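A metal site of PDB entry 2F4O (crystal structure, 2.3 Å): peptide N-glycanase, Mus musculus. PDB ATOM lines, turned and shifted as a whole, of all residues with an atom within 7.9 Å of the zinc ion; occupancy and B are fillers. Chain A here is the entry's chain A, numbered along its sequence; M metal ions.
The side-chain sulfur (SG) of Cys 87 lies close to the backbone NH (N) of Gly 89 (3.5 Å). The backbone NH (N) of Cys 117 is in hydrogen-bond range of the backbone carbonyl oxygen (O) of Leu 122 (2.9 Å). The side-chain sulfur of Cys 84 lies close to the backbone NH of Lys 86, 3.3 Å away. The backbone carbonyl oxygen of Gly 89 lies within hydrogen-bond range of the backbone NH of Cys 84, 3.0 Å away. The side-chain sulfur (SG) of Cys 84 sits close to the side-chain amide nitrogen (ND2) of Asn 124, 3.8 Å away.
Of the 17 residues printed, 4 come within 4 Å of the zinc ion. Along chain A the residues within 4 Å of the zinc ion span positions 84 to 120.
The zinc ion is bound by the side-chain sulfur of Cys 87 (2.2 Å), the side-chain sulfur of Cys 117 (2.3 Å), the side-chain sulfur of Cys 120 (2.3 Å) and the side-chain sulfur of Cys 84 (2.5 Å). The zinc ion has four donor atoms within binding distance.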
ATOM      1  N   VAL A  83     -16.588  -6.981  10.669  1.00  0.00           N
ATOM      2  CA  VAL A  83     -16.057  -8.287  10.270  1.00  0.00           C
ATOM      3  C   VAL A  83     -16.099  -8.392   8.757  1.00  0.00           C
ATOM      4  O   VAL A  83     -16.921  -7.743   8.089  1.00  0.00           O
ATOM      5  CB  VAL A  83     -16.871  -9.509  10.843  1.00  0.00           C
ATOM      6  CG1 VAL A  83     -16.865  -9.539  12.358  1.00  0.00           C
ATOM      7  CG2 VAL A  83     -18.321  -9.550  10.311  1.00  0.00           C
ATOM      8  N   CYS A  84     -15.216  -9.227   8.233  1.00  0.00           N
ATOM      9  CA  CYS A  84     -15.127  -9.378   6.799  1.00  0.00           C
ATOM     10  C   CYS A  84     -16.385 -10.002   6.166  1.00  0.00           C
ATOM     11  O   CYS A  84     -16.858 -11.065   6.594  1.00  0.00           O
ATOM     12  CB  CYS A  84     -13.907 -10.215   6.444  1.00  0.00           C
ATOM     13  SG  CYS A  84     -13.756 -10.447   4.676  1.00  0.00           S
ATOM     14  N   SER A  85     -16.896  -9.328   5.144  1.00  0.00           N
ATOM     15  CA  SER A  85     -18.072  -9.793   4.421  1.00  0.00           C
ATOM     16  C   SER A  85     -17.837 -11.196   3.877  1.00  0.00           C
ATOM     17  O   SER A  85     -18.728 -12.060   3.914  1.00  0.00           O
ATOM     18  CB  SER A  85     -18.435  -8.839   3.268  1.00  0.00           C
ATOM     19  OG  SER A  85     -17.332  -8.574   2.410  1.00  0.00           O
ATOM     20  N   LYS A  86     -16.625 -11.414   3.381  1.00  0.00           N
ATOM     21  CA  LYS A  86     -16.277 -12.645   2.688  1.00  0.00           C
ATOM     22  C   LYS A  86     -16.054 -13.765   3.719  1.00  0.00           C
ATOM     23  O   LYS A  86     -16.861 -14.699   3.772  1.00  0.00           O
ATOM     24  CB  LYS A  86     -15.017 -12.394   1.820  1.00  0.00           C
ATOM     25  CG  LYS A  86     -14.792 -13.378   0.651  1.00  0.00           C
ATOM     26  CD  LYS A  86     -15.529 -12.911  -0.628  1.00  0.00           C
ATOM     27  CE  LYS A  86     -15.089 -13.656  -1.832  1.00  0.00           C
ATOM     28  NZ  LYS A  86     -15.166 -15.121  -1.620  1.00  0.00           N
ATOM     29  N   CYS A  87     -15.019 -13.644   4.555  1.00  0.00           N
ATOM     30  CA  CYS A  87     -14.576 -14.726   5.456  1.00  0.00           C
ATOM     31  C   CYS A  87     -15.061 -14.618   6.878  1.00  0.00           C
ATOM     32  O   CYS A  87     -14.881 -15.563   7.640  1.00  0.00           O
ATOM     33  CB  CYS A  87     -13.063 -14.777   5.503  1.00  0.00           C
ATOM     34  SG  CYS A  87     -12.292 -13.410   6.416  1.00  0.00           S
ATOM     35  N   GLY A  88     -15.591 -13.468   7.273  1.00  0.00           N
ATOM     36  CA  GLY A  88     -16.211 -13.293   8.585  1.00  0.00           C
ATOM     37  C   GLY A  88     -15.257 -12.986   9.722  1.00  0.00           C
ATOM     38  O   GLY A  88     -15.684 -12.872  10.886  1.00  0.00           O
ATOM     39  N   GLY A  89     -13.971 -12.831   9.389  1.00  0.00           N
ATOM     40  CA  GLY A  89     -12.908 -12.642  10.375  1.00  0.00           C
ATOM     41  C   GLY A  89     -12.503 -11.204  10.613  1.00  0.00           C
ATOM     42  O   GLY A  89     -13.007 -10.292   9.955  1.00  0.00           O
ATOM     43  N   GLU A  90     -11.632 -11.022  11.609  1.00  0.00           N
ATOM     44  CA  GLU A  90     -10.880  -9.788  11.883  1.00  0.00           C
ATOM     45  C   GLU A  90     -10.582  -8.899  10.680  1.00  0.00           C
ATOM     46  O   GLU A  90     -10.139  -9.398   9.638  1.00  0.00           O
ATOM     47  CB  GLU A  90      -9.518 -10.169  12.484  1.00  0.00           C
ATOM     48  CG  GLU A  90      -8.826 -11.345  11.728  1.00  0.00           C
ATOM     49  CD  GLU A  90      -7.308 -11.185  11.549  1.00  0.00           C
ATOM     50  OE1 GLU A  90      -6.843 -10.046  11.269  1.00  0.00           O
ATOM     51  OE2 GLU A  90      -6.589 -12.197  11.681  1.00  0.00           O
ATOM     52  N   THR A  91     -10.795  -7.592  10.847  1.00  0.00           N
ATOM     53  CA  THR A  91     -10.279  -6.588   9.912  1.00  0.00           C
ATOM     54  C   THR A  91      -9.496  -5.480  10.653  1.00  0.00           C
ATOM     55  O   THR A  91      -9.552  -5.371  11.869  1.00  0.00           O
ATOM     56  CB  THR A  91     -11.401  -5.946   9.047  1.00  0.00           C
ATOM     57  OG1 THR A  91     -12.272  -5.157   9.874  1.00  0.00           O
ATOM     58  CG2 THR A  91     -12.219  -7.032   8.313  1.00  0.00           C
ATOM     59  N   TYR A 116      -9.821  -3.375   6.350  1.00  0.00           N
ATOM     60  CA  TYR A 116      -9.136  -4.286   5.455  1.00  0.00           C
ATOM     61  C   TYR A 116      -9.047  -5.659   6.095  1.00  0.00           C
ATOM     62  O   TYR A 116      -8.702  -5.790   7.281  1.00  0.00           O
ATOM     63  CB  TYR A 116      -7.748  -3.765   5.046  1.00  0.00           C
ATOM     64  CG  TYR A 116      -7.356  -4.205   3.650  1.00  0.00           C
ATOM     65  CD1 TYR A 116      -7.947  -3.604   2.535  1.00  0.00           C
ATOM     66  CD2 TYR A 116      -6.433  -5.214   3.423  1.00  0.00           C
ATOM     67  CE1 TYR A 116      -7.616  -3.999   1.223  1.00  0.00           C
ATOM     68  CE2 TYR A 116      -6.094  -5.630   2.103  1.00  0.00           C
ATOM     69  CZ  TYR A 116      -6.708  -5.008   1.016  1.00  0.00           C
ATOM     70  OH  TYR A 116      -6.414  -5.367  -0.279  1.00  0.00           O
ATOM     71  N   CYS A 117      -9.372  -6.669   5.287  1.00  0.00           N
ATOM     72  CA  CYS A 117      -9.027  -8.060   5.550  1.00  0.00           C
ATOM     73  C   CYS A 117      -7.731  -8.399   4.813  1.00  0.00           C
ATOM     74  O   CYS A 117      -7.683  -8.346   3.581  1.00  0.00           O
ATOM     75  CB  CYS A 117     -10.165  -8.948   5.063  1.00  0.00           C
ATOM     76  SG  CYS A 117     -10.027 -10.621   5.625  1.00  0.00           S
ATOM     77  N   ASP A 118      -6.673  -8.749   5.545  1.00  0.00           N
ATOM     78  CA  ASP A 118      -5.397  -9.197   4.930  1.00  0.00           C
ATOM     79  C   ASP A 118      -5.517 -10.597   4.276  1.00  0.00           C
ATOM     80  O   ASP A 118      -4.933 -10.870   3.226  1.00  0.00           O
ATOM     81  CB  ASP A 118      -4.244  -9.183   5.957  1.00  0.00           C
ATOM     82  CG  ASP A 118      -4.031  -7.804   6.607  1.00  0.00           C
ATOM     83  OD1 ASP A 118      -3.696  -6.836   5.874  1.00  0.00           O
ATOM     84  OD2 ASP A 118      -4.195  -7.701   7.857  1.00  0.00           O
ATOM     85  N   ALA A 119      -6.266 -11.477   4.923  1.00  0.00           N
ATOM     86  CA  ALA A 119      -6.537 -12.802   4.428  1.00  0.00           C
ATOM     87  C   ALA A 119      -7.196 -12.748   3.046  1.00  0.00           C
ATOM     88  O   ALA A 119      -6.737 -13.378   2.120  1.00  0.00           O
ATOM     89  CB  ALA A 119      -7.397 -13.565   5.406  1.00  0.00           C
ATOM     90  N   CYS A 120      -8.261 -11.970   2.911  1.00  0.00           N
ATOM     91  CA  CYS A 120      -9.041 -11.926   1.673  1.00  0.00           C
ATOM     92  C   CYS A 120      -8.537 -10.837   0.715  1.00  0.00           C
ATOM     93  O   CYS A 120      -8.983 -10.775  -0.434  1.00  0.00           O
ATOM     94  CB  CYS A 120     -10.532 -11.721   1.983  1.00  0.00           C
ATOM     95  SG  CYS A 120     -11.383 -13.096   2.850  1.00  0.00           S
ATOM     96  N   GLN A 121      -7.610  -9.979   1.162  1.00  0.00           N
ATOM     97  CA  GLN A 121      -7.217  -8.786   0.385  1.00  0.00           C
ATOM     98  C   GLN A 121      -8.507  -8.045  -0.022  1.00  0.00           C
ATOM     99  O   GLN A 121      -8.677  -7.664  -1.176  1.00  0.00           O
ATOM    100  CB  GLN A 121      -6.380  -9.177  -0.848  1.00  0.00           C
ATOM    101  CG  GLN A 121      -4.904  -8.826  -0.806  1.00  0.00           C
ATOM    102  CD  GLN A 121      -4.184  -9.416   0.396  1.00  0.00           C
ATOM    103  OE1 GLN A 121      -4.206  -8.843   1.499  1.00  0.00           O
ATOM    104  NE2 GLN A 121      -3.501 -10.539   0.180  1.00  0.00           N
ATOM    105  N   LEU A 122      -9.391  -7.867   0.954  1.00  0.00           N
ATOM    106  CA  LEU A 122     -10.714  -7.310   0.751  1.00  0.00           C
ATOM    107  C   LEU A 122     -10.875  -6.059   1.635  1.00  0.00           C
ATOM    108  O   LEU A 122     -10.767  -6.126   2.855  1.00  0.00           O
ATOM    109  CB  LEU A 122     -11.772  -8.369   1.126  1.00  0.00           C
ATOM    110  CG  LEU A 122     -13.275  -8.083   0.881  1.00  0.00           C
ATOM    111  CD1 LEU A 122     -13.709  -8.109  -0.586  1.00  0.00           C
ATOM    112  CD2 LEU A 122     -14.098  -9.116   1.608  1.00  0.00           C
ATOM    113  N   ASN A 124     -13.395  -3.895   3.337  1.00  0.00           N
ATOM    114  CA  ASN A 124     -14.777  -3.790   3.847  1.00  0.00           C
ATOM    115  C   ASN A 124     -15.085  -2.323   4.184  1.00  0.00           C
ATOM    116  O   ASN A 124     -14.217  -1.545   4.550  1.00  0.00           O
ATOM    117  CB  ASN A 124     -15.005  -4.707   5.066  1.00  0.00           C
ATOM    118  CG  ASN A 124     -14.873  -6.197   4.709  1.00  0.00           C
ATOM    119  OD1 ASN A 124     -15.872  -6.891   4.514  1.00  0.00           O
ATOM    120  ND2 ASN A 124     -13.648  -6.678   4.623  1.00  0.00           N
HETATM  121 ZN    ZN M   1     -11.720 -11.923   4.848  1.00  0.00          ZN
